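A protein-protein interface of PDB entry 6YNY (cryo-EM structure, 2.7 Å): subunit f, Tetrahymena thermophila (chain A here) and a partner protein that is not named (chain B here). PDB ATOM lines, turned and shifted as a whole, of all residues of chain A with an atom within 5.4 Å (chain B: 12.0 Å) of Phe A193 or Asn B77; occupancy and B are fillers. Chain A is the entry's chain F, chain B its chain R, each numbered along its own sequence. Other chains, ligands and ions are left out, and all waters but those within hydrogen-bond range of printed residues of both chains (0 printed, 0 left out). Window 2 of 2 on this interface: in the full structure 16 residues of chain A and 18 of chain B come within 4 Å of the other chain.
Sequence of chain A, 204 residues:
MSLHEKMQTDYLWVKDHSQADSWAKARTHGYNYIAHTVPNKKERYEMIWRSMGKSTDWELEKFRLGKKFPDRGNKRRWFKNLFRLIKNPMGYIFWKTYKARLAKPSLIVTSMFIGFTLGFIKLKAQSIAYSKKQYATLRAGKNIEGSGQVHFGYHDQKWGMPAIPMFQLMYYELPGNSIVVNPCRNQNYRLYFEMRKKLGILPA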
ATOM      1  N   TYR A 189     -18.852  14.768  29.080  1.00  0.00           N
ATOM      2  CA  TYR A 189     -18.486  15.263  27.764  1.00  0.00           C
ATOM      3  C   TYR A 189     -18.030  14.145  26.842  1.00  0.00           C
ATOM      4  O   TYR A 189     -17.989  14.340  25.624  1.00  0.00           O
ATOM      5  CB  TYR A 189     -17.390  16.317  27.895  1.00  0.00           C
ATOM      6  CG  TYR A 189     -17.892  17.651  28.380  1.00  0.00           C
ATOM      7  CD1 TYR A 189     -18.123  17.879  29.723  1.00  0.00           C
ATOM      8  CD2 TYR A 189     -18.137  18.680  27.492  1.00  0.00           C
ATOM      9  CE1 TYR A 189     -18.585  19.091  30.165  1.00  0.00           C
ATOM     10  CE2 TYR A 189     -18.599  19.897  27.924  1.00  0.00           C
ATOM     11  CZ  TYR A 189     -18.821  20.100  29.262  1.00  0.00           C
ATOM     12  OH  TYR A 189     -19.283  21.318  29.696  1.00  0.00           O
ATOM     13  N   ARG A 190     -17.685  12.985  27.396  1.00  0.00           N
ATOM     14  CA  ARG A 190     -17.344  11.839  26.564  1.00  0.00           C
ATOM     15  C   ARG A 190     -18.504  11.458  25.658  1.00  0.00           C
ATOM     16  O   ARG A 190     -18.297  11.032  24.516  1.00  0.00           O
ATOM     17  CB  ARG A 190     -16.948  10.661  27.446  1.00  0.00           C
ATOM     18  CG  ARG A 190     -15.830  10.963  28.417  1.00  0.00           C
ATOM     19  CD  ARG A 190     -15.505   9.762  29.270  1.00  0.00           C
ATOM     20  NE  ARG A 190     -14.414  10.022  30.198  1.00  0.00           N
ATOM     21  CZ  ARG A 190     -13.707   9.074  30.800  1.00  0.00           C
ATOM     22  NH1 ARG A 190     -13.964   7.799  30.570  1.00  0.00           N
ATOM     23  NH2 ARG A 190     -12.735   9.402  31.629  1.00  0.00           N
ATOM     24  N   LEU A 191     -19.734  11.603  26.150  1.00  0.00           N
ATOM     25  CA  LEU A 191     -20.903  11.350  25.318  1.00  0.00           C
ATOM     26  C   LEU A 191     -20.907  12.239  24.085  1.00  0.00           C
ATOM     27  O   LEU A 191     -21.289  11.801  22.994  1.00  0.00           O
ATOM     28  CB  LEU A 191     -22.173  11.578  26.131  1.00  0.00           C
ATOM     29  CG  LEU A 191     -22.380  10.680  27.341  1.00  0.00           C
ATOM     30  CD1 LEU A 191     -23.417  11.273  28.261  1.00  0.00           C
ATOM     31  CD2 LEU A 191     -22.805   9.309  26.892  1.00  0.00           C
ATOM     32  N   TYR A 192     -20.491  13.494  24.239  1.00  0.00           N
ATOM     33  CA  TYR A 192     -20.508  14.418  23.114  1.00  0.00           C
ATOM     34  C   TYR A 192     -19.481  14.023  22.064  1.00  0.00           C
ATOM     35  O   TYR A 192     -19.765  14.066  20.862  1.00  0.00           O
ATOM     36  CB  TYR A 192     -20.251  15.841  23.605  1.00  0.00           C
ATOM     37  CG  TYR A 192     -21.147  16.284  24.736  1.00  0.00           C
ATOM     38  CD1 TYR A 192     -20.775  17.320  25.573  1.00  0.00           C
ATOM     39  CD2 TYR A 192     -22.364  15.670  24.966  1.00  0.00           C
ATOM     40  CE1 TYR A 192     -21.585  17.729  26.602  1.00  0.00           C
ATOM     41  CE2 TYR A 192     -23.178  16.070  25.995  1.00  0.00           C
ATOM     42  CZ  TYR A 192     -22.786  17.100  26.810  1.00  0.00           C
ATOM     43  OH  TYR A 192     -23.603  17.503  27.835  1.00  0.00           O
ATOM     44  N   PHE A 193     -18.283  13.639  22.497  1.00  0.00           N
ATOM     45  CA  PHE A 193     -17.245  13.245  21.556  1.00  0.00           C
ATOM     46  C   PHE A 193     -17.623  11.983  20.800  1.00  0.00           C
ATOM     47  O   PHE A 193     -17.242  11.821  19.636  1.00  0.00           O
ATOM     48  CB  PHE A 193     -15.927  13.048  22.299  1.00  0.00           C
ATOM     49  CG  PHE A 193     -15.506  14.238  23.102  1.00  0.00           C
ATOM     50  CD1 PHE A 193     -15.698  15.516  22.623  1.00  0.00           C
ATOM     51  CD2 PHE A 193     -14.930  14.081  24.345  1.00  0.00           C
ATOM     52  CE1 PHE A 193     -15.318  16.605  23.358  1.00  0.00           C
ATOM     53  CE2 PHE A 193     -14.548  15.172  25.084  1.00  0.00           C
ATOM     54  CZ  PHE A 193     -14.743  16.435  24.590  1.00  0.00           C
ATOM     55  N   GLU A 194     -18.367  11.081  21.437  1.00  0.00           N
ATOM     56  CA  GLU A 194     -18.779   9.852  20.772  1.00  0.00           C
ATOM     57  C   GLU A 194     -19.928  10.096  19.803  1.00  0.00           C
ATOM     58  O   GLU A 194     -19.995   9.459  18.746  1.00  0.00           O
ATOM     59  CB  GLU A 194     -19.168   8.811  21.816  1.00  0.00           C
ATOM     60  CG  GLU A 194     -18.030   8.421  22.738  1.00  0.00           C
ATOM     61  CD  GLU A 194     -18.487   7.581  23.912  1.00  0.00           C
ATOM     62  OE1 GLU A 194     -19.667   7.173  23.933  1.00  0.00           O
ATOM     63  OE2 GLU A 194     -17.667   7.331  24.819  1.00  0.00           O
ATOM     64  N   MET A 195     -20.837  11.008  20.143  1.00  0.00           N
ATOM     65  CA  MET A 195     -21.935  11.329  19.238  1.00  0.00           C
ATOM     66  C   MET A 195     -21.429  12.047  17.997  1.00  0.00           C
ATOM     67  O   MET A 195     -21.882  11.767  16.882  1.00  0.00           O
ATOM     68  CB  MET A 195     -22.972  12.184  19.961  1.00  0.00           C
ATOM     69  CG  MET A 195     -24.166  12.584  19.110  1.00  0.00           C
ATOM     70  SD  MET A 195     -25.290  11.227  18.756  1.00  0.00           S
ATOM     71  CE  MET A 195     -26.158  11.132  20.314  1.00  0.00           C
ATOM     72  N   ARG A 196     -20.490  12.977  18.170  1.00  0.00           N
ATOM     73  CA  ARG A 196     -19.956  13.712  17.031  1.00  0.00           C
ATOM     74  C   ARG A 196     -19.347  12.771  16.003  1.00  0.00           C
ATOM     75  O   ARG A 196     -19.451  13.009  14.795  1.00  0.00           O
ATOM     76  CB  ARG A 196     -18.924  14.727  17.510  1.00  0.00           C
ATOM     77  CG  ARG A 196     -19.524  15.864  18.297  1.00  0.00           C
ATOM     78  CD  ARG A 196     -18.476  16.649  19.049  1.00  0.00           C
ATOM     79  NE  ARG A 196     -17.472  17.234  18.168  1.00  0.00           N
ATOM     80  CZ  ARG A 196     -17.608  18.397  17.540  1.00  0.00           C
ATOM     81  NH1 ARG A 196     -16.636  18.841  16.762  1.00  0.00           N
ATOM     82  NH2 ARG A 196     -18.712  19.111  17.678  1.00  0.00           N
ATOM     83  N   LYS A 197     -18.705  11.699  16.460  1.00  0.00           N
ATOM     84  CA  LYS A 197     -18.119  10.740  15.535  1.00  0.00           C
ATOM     85  C   LYS A 197     -19.171   9.853  14.893  1.00  0.00           C
ATOM     86  O   LYS A 197     -19.015   9.453  13.735  1.00  0.00           O
ATOM     87  CB  LYS A 197     -17.083   9.882  16.256  1.00  0.00           C
ATOM     88  CG  LYS A 197     -15.873  10.652  16.712  1.00  0.00           C
ATOM     89  CD  LYS A 197     -14.741   9.730  17.081  1.00  0.00           C
ATOM     90  CE  LYS A 197     -13.467  10.507  17.311  1.00  0.00           C
ATOM     91  NZ  LYS A 197     -12.307   9.623  17.545  1.00  0.00           N
ATOM     92  N   ALA B  66      -5.453  25.829  20.870  1.00  0.00           N
ATOM     93  CA  ALA B  66      -5.075  25.163  22.110  1.00  0.00           C
ATOM     94  C   ALA B  66      -6.297  24.699  22.886  1.00  0.00           C
ATOM     95  O   ALA B  66      -6.266  23.645  23.530  1.00  0.00           O
ATOM     96  CB  ALA B  66      -4.225  26.098  22.961  1.00  0.00           C
ATOM     97  N   VAL B  67      -7.379  25.474  22.847  1.00  0.00           N
ATOM     98  CA  VAL B  67      -8.612  25.064  23.511  1.00  0.00           C
ATOM     99  C   VAL B  67      -9.128  23.766  22.906  1.00  0.00           C
ATOM    100  O   VAL B  67      -9.479  22.822  23.622  1.00  0.00           O
ATOM    101  CB  VAL B  67      -9.658  26.187  23.424  1.00  0.00           C
ATOM    102  CG1 VAL B  67     -11.010  25.698  23.873  1.00  0.00           C
ATOM    103  CG2 VAL B  67      -9.234  27.357  24.266  1.00  0.00           C
ATOM    104  N   ASP B  68      -9.177  23.697  21.576  1.00  0.00           N
ATOM    105  CA  ASP B  68      -9.611  22.470  20.919  1.00  0.00           C
ATOM    106  C   ASP B  68      -8.674  21.314  21.238  1.00  0.00           C
ATOM    107  O   ASP B  68      -9.119  20.177  21.424  1.00  0.00           O
ATOM    108  CB  ASP B  68      -9.698  22.695  19.413  1.00  0.00           C
ATOM    109  CG  ASP B  68     -10.798  23.662  19.035  1.00  0.00           C
ATOM    110  OD1 ASP B  68     -10.678  24.859  19.365  1.00  0.00           O
ATOM    111  OD2 ASP B  68     -11.785  23.225  18.411  1.00  0.00           O
ATOM    112  N   LYS B  69      -7.372  21.589  21.304  1.00  0.00           N
ATOM    113  CA  LYS B  69      -6.412  20.572  21.712  1.00  0.00           C
ATOM    114  C   LYS B  69      -6.637  20.146  23.156  1.00  0.00           C
ATOM    115  O   LYS B  69      -6.355  19.000  23.519  1.00  0.00           O
ATOM    116  CB  LYS B  69      -4.998  21.112  21.521  1.00  0.00           C
ATOM    117  CG  LYS B  69      -3.877  20.196  21.949  1.00  0.00           C
ATOM    118  CD  LYS B  69      -3.689  19.058  20.987  1.00  0.00           C
ATOM    119  CE  LYS B  69      -2.523  18.181  21.400  1.00  0.00           C
ATOM    120  NZ  LYS B  69      -1.261  18.956  21.533  1.00  0.00           N
ATOM    121  N   TYR B  70      -7.144  21.054  23.989  1.00  0.00           N
ATOM    122  CA  TYR B  70      -7.359  20.759  25.398  1.00  0.00           C
ATOM    123  C   TYR B  70      -8.662  20.014  25.631  1.00  0.00           C
ATOM    124  O   TYR B  70      -8.760  19.222  26.574  1.00  0.00           O
ATOM    125  CB  TYR B  70      -7.346  22.064  26.196  1.00  0.00           C
ATOM    126  CG  TYR B  70      -7.659  21.930  27.664  1.00  0.00           C
ATOM    127  CD1 TYR B  70      -6.721  21.432  28.549  1.00  0.00           C
ATOM    128  CD2 TYR B  70      -8.886  22.325  28.170  1.00  0.00           C
ATOM    129  CE1 TYR B  70      -6.999  21.317  29.891  1.00  0.00           C
ATOM    130  CE2 TYR B  70      -9.172  22.214  29.508  1.00  0.00           C
ATOM    131  CZ  TYR B  70      -8.225  21.709  30.365  1.00  0.00           C
ATOM    132  OH  TYR B  70      -8.505  21.596  31.706  1.00  0.00           O
ATOM    133  N   ILE B  71      -9.662  20.249  24.790  1.00  0.00           N
ATOM    134  CA  ILE B  71     -10.978  19.652  24.971  1.00  0.00           C
ATOM    135  C   ILE B  71     -11.123  18.372  24.166  1.00  0.00           C
ATOM    136  O   ILE B  71     -11.557  17.343  24.688  1.00  0.00           O
ATOM    137  CB  ILE B  71     -12.066  20.680  24.597  1.00  0.00           C
ATOM    138  CG1 ILE B  71     -12.051  21.840  25.587  1.00  0.00           C
ATOM    139  CG2 ILE B  71     -13.425  20.020  24.561  1.00  0.00           C
ATOM    140  CD1 ILE B  71     -12.900  22.994  25.181  1.00  0.00           C
ATOM    141  N   PHE B  72     -10.760  18.414  22.886  1.00  0.00           N
ATOM    142  CA  PHE B  72     -10.948  17.277  21.999  1.00  0.00           C
ATOM    143  C   PHE B  72      -9.747  16.345  21.979  1.00  0.00           C
ATOM    144  O   PHE B  72      -9.914  15.126  21.868  1.00  0.00           O
ATOM    145  CB  PHE B  72     -11.240  17.772  20.584  1.00  0.00           C
ATOM    146  CG  PHE B  72     -12.469  18.616  20.488  1.00  0.00           C
ATOM    147  CD1 PHE B  72     -13.709  18.037  20.325  1.00  0.00           C
ATOM    148  CD2 PHE B  72     -12.386  19.990  20.567  1.00  0.00           C
ATOM    149  CE1 PHE B  72     -14.837  18.812  20.240  1.00  0.00           C
ATOM    150  CE2 PHE B  72     -13.513  20.765  20.481  1.00  0.00           C
ATOM    151  CZ  PHE B  72     -14.738  20.175  20.318  1.00  0.00           C
ATOM    152  N   GLY B  73      -8.542  16.889  22.083  1.00  0.00           N
ATOM    153  CA  GLY B  73      -7.354  16.066  22.113  1.00  0.00           C
ATOM    154  C   GLY B  73      -6.741  15.836  20.750  1.00  0.00           C
ATOM    155  O   GLY B  73      -6.840  16.683  19.858  1.00  0.00           O
ATOM    156  N   GLU B  74      -6.101  14.681  20.585  1.00  0.00           N
ATOM    157  CA  GLU B  74      -5.407  14.372  19.343  1.00  0.00           C
ATOM    158  C   GLU B  74      -6.374  13.903  18.264  1.00  0.00           C
ATOM    159  O   GLU B  74      -6.311  14.365  17.121  1.00  0.00           O
ATOM    160  CB  GLU B  74      -4.346  13.300  19.589  1.00  0.00           C
ATOM    161  CG  GLU B  74      -3.439  13.561  20.773  1.00  0.00           C
ATOM    162  CD  GLU B  74      -2.593  14.804  20.602  1.00  0.00           C
ATOM    163  OE1 GLU B  74      -2.592  15.378  19.493  1.00  0.00           O
ATOM    164  OE2 GLU B  74      -1.928  15.209  21.578  1.00  0.00           O
ATOM    165  N   ASN B  75      -7.272  12.984  18.609  1.00  0.00           N
ATOM    166  CA  ASN B  75      -8.146  12.330  17.645  1.00  0.00           C
ATOM    167  C   ASN B  75      -9.616  12.515  17.999  1.00  0.00           C
ATOM    168  O   ASN B  75     -10.442  11.625  17.788  1.00  0.00           O
ATOM    169  CB  ASN B  75      -7.804  10.849  17.540  1.00  0.00           C
ATOM    170  CG  ASN B  75      -8.296  10.232  16.260  1.00  0.00           C
ATOM    171  OD1 ASN B  75      -8.407  10.903  15.236  1.00  0.00           O
ATOM    172  ND2 ASN B  75      -8.597   8.947  16.308  1.00  0.00           N
ATOM    173  N   GLY B  76      -9.963  13.674  18.546  1.00  0.00           N
ATOM    174  CA  GLY B  76     -11.356  13.984  18.803  1.00  0.00           C
ATOM    175  C   GLY B  76     -12.037  13.101  19.818  1.00  0.00           C
ATOM    176  O   GLY B  76     -13.263  12.980  19.792  1.00  0.00           O
ATOM    177  N   ASN B  77     -11.280  12.483  20.719  1.00  0.00           N
ATOM    178  CA  ASN B  77     -11.837  11.631  21.758  1.00  0.00           C
ATOM    179  C   ASN B  77     -11.747  12.244  23.145  1.00  0.00           C
ATOM    180  O   ASN B  77     -12.226  11.635  24.107  1.00  0.00           O
ATOM    181  CB  ASN B  77     -11.133  10.272  21.755  1.00  0.00           C
ATOM    182  CG  ASN B  77     -11.465   9.450  20.539  1.00  0.00           C
ATOM    183  OD1 ASN B  77     -12.589   9.477  20.043  1.00  0.00           O
ATOM    184  ND2 ASN B  77     -10.486   8.709  20.048  1.00  0.00           N
ATOM    185  N   GLY B  78     -11.157  13.426  23.277  1.00  0.00           N
ATOM    186  CA  GLY B  78     -11.010  14.058  24.569  1.00  0.00           C
ATOM    187  C   GLY B  78      -9.568  14.308  24.945  1.00  0.00           C
ATOM    188  O   GLY B  78      -8.703  13.451  24.746  1.00  0.00           O
ATOM    189  N   GLY B  79      -9.303  15.488  25.495  1.00  0.00           N
ATOM    190  CA  GLY B  79      -7.967  15.868  25.894  1.00  0.00           C
ATOM    191  C   GLY B  79      -7.765  15.892  27.392  1.00  0.00           C
ATOM    192  O   GLY B  79      -8.424  15.159  28.134  1.00  0.00           O
ATOM    193  N   LYS B  80      -6.844  16.741  27.847  1.00  0.00           N
ATOM    194  CA  LYS B  80      -6.565  16.873  29.269  1.00  0.00           C
ATOM    195  C   LYS B  80      -7.724  17.481  30.041  1.00  0.00           C
ATOM    196  O   LYS B  80      -7.684  17.495  31.274  1.00  0.00           O
ATOM    197  CB  LYS B  80      -5.312  17.716  29.469  1.00  0.00           C
ATOM    198  CG  LYS B  80      -4.075  17.092  28.884  1.00  0.00           C
ATOM    199  CD  LYS B  80      -2.843  17.901  29.209  1.00  0.00           C
ATOM    200  CE  LYS B  80      -1.616  17.317  28.541  1.00  0.00           C
ATOM    201  NZ  LYS B  80      -0.384  18.065  28.889  1.00  0.00           N
ATOM    202  N   PHE B  81      -8.745  17.982  29.351  1.00  0.00           N
ATOM    203  CA  PHE B  81      -9.921  18.495  30.040  1.00  0.00           C
ATOM    204  C   PHE B  81     -10.594  17.409  30.865  1.00  0.00           C
ATOM    205  O   PHE B  81     -11.255  17.709  31.865  1.00  0.00           O
ATOM    206  CB  PHE B  81     -10.894  19.081  29.020  1.00  0.00           C
ATOM    207  CG  PHE B  81     -12.259  19.334  29.562  1.00  0.00           C
ATOM    208  CD1 PHE B  81     -13.325  18.556  29.163  1.00  0.00           C
ATOM    209  CD2 PHE B  81     -12.481  20.348  30.469  1.00  0.00           C
ATOM    210  CE1 PHE B  81     -14.580  18.783  29.656  1.00  0.00           C
ATOM    211  CE2 PHE B  81     -13.739  20.579  30.967  1.00  0.00           C
ATOM    212  CZ  PHE B  81     -14.790  19.795  30.559  1.00  0.00           C
ATOM    213  N   LEU B  82     -10.430  16.150  30.471  1.00  0.00           N
ATOM    214  CA  LEU B  82     -11.036  15.025  31.163  1.00  0.00           C
ATOM    215  C   LEU B  82     -10.186  14.495  32.307  1.00  0.00           C
ATOM    216  O   LEU B  82     -10.639  13.604  33.031  1.00  0.00           O
ATOM    217  CB  LEU B  82     -11.298  13.890  30.173  1.00  0.00           C
ATOM    218  CG  LEU B  82     -12.196  14.234  28.990  1.00  0.00           C
ATOM    219  CD1 LEU B  82     -12.162  13.119  27.979  1.00  0.00           C
ATOM    220  CD2 LEU B  82     -13.610  14.483  29.457  1.00  0.00           C
ATOM    221  N   GLU B  83      -8.975  15.009  32.486  1.00  0.00           N
ATOM    222  CA  GLU B  83      -8.083  14.526  33.526  1.00  0.00           C
ATOM    223  C   GLU B  83      -8.339  15.261  34.832  1.00  0.00           C
ATOM    224  O   GLU B  83      -8.493  16.484  34.854  1.00  0.00           O
ATOM    225  CB  GLU B  83      -6.623  14.706  33.112  1.00  0.00           C
ATOM    226  CG  GLU B  83      -6.256  13.985  31.839  1.00  0.00           C
ATOM    227  CD  GLU B  83      -4.821  14.226  31.432  1.00  0.00           C
ATOM    228  OE1 GLU B  83      -4.092  14.892  32.194  1.00  0.00           O
ATOM    229  OE2 GLU B  83      -4.421  13.749  30.349  1.00  0.00           O
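OD1 of Asn B77 lies within hydrogen-bond range of NZ of Lys A197.
NZ of Lys A197 lies within hydrogen-bond range of O of Asn B75, 2.7 Å away.
The backbone NH (N) of Phe B81 sits at hydrogen-bond distance from the backbone carbonyl oxygen (O) of Tyr B70 (3.0 Å).
The backbone carbonyl oxygen (O) of Ile B71 sits at hydrogen-bond distance from the backbone NH (N) of Gly B79.
N of Gly B78 sits at hydrogen-bond distance from O of Phe B72.
O of Phe B72 sits at hydrogen-bond distance from N of Asn B77.
Among the printed residues, merely in contact across the chains: Tyr A189 with Phe B81, Phe A193 with Ile B71, Phe A193 with Phe B72, Phe A193 with Gly B76, Phe A193 with Asn B77, Phe A193 with Gly B78, Arg A196 with Phe B72 and Lys A197 with Gly B76.
Arg A190 touches none of the printed residues of chain B.
Tyr A192 touches none of the printed residues of chain B.
Phe A193 touches just these residues of chain B: Ile B71, Phe B72, Gly B76, Asn B77 and Gly B78.
No residue of chain B comes within 4 Å of Glu A194.
Of chain B, only Phe B72 comes within 4 Å of Arg A196.
Lys A197 touches just these residues of chain B: Asn B75, Gly B76 and Asn B77.
Tyr B70 touches none of the printed residues of chain A.
Of the printed residues of chain A, Ile B71 touches Phe A193.
Printed residues of chain A within 4 Å of Asn B75: Lys A197.
Asn B77 touches just these residues of chain A: Phe A193 (3.7 Å) and Lys A197 (2.5 Å).
Of the printed residues of chain A, Phe B81 touches Tyr A189 (3.7 Å).
The nearest printed residue of chain A that does not touch Asn B77 is Arg A190 (5.7 Å).
Of the 9 printed residues of chain A, 4 touch a printed residue of chain B.
Of the 18 printed residues of chain B, 7 touch a printed residue of chain A.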
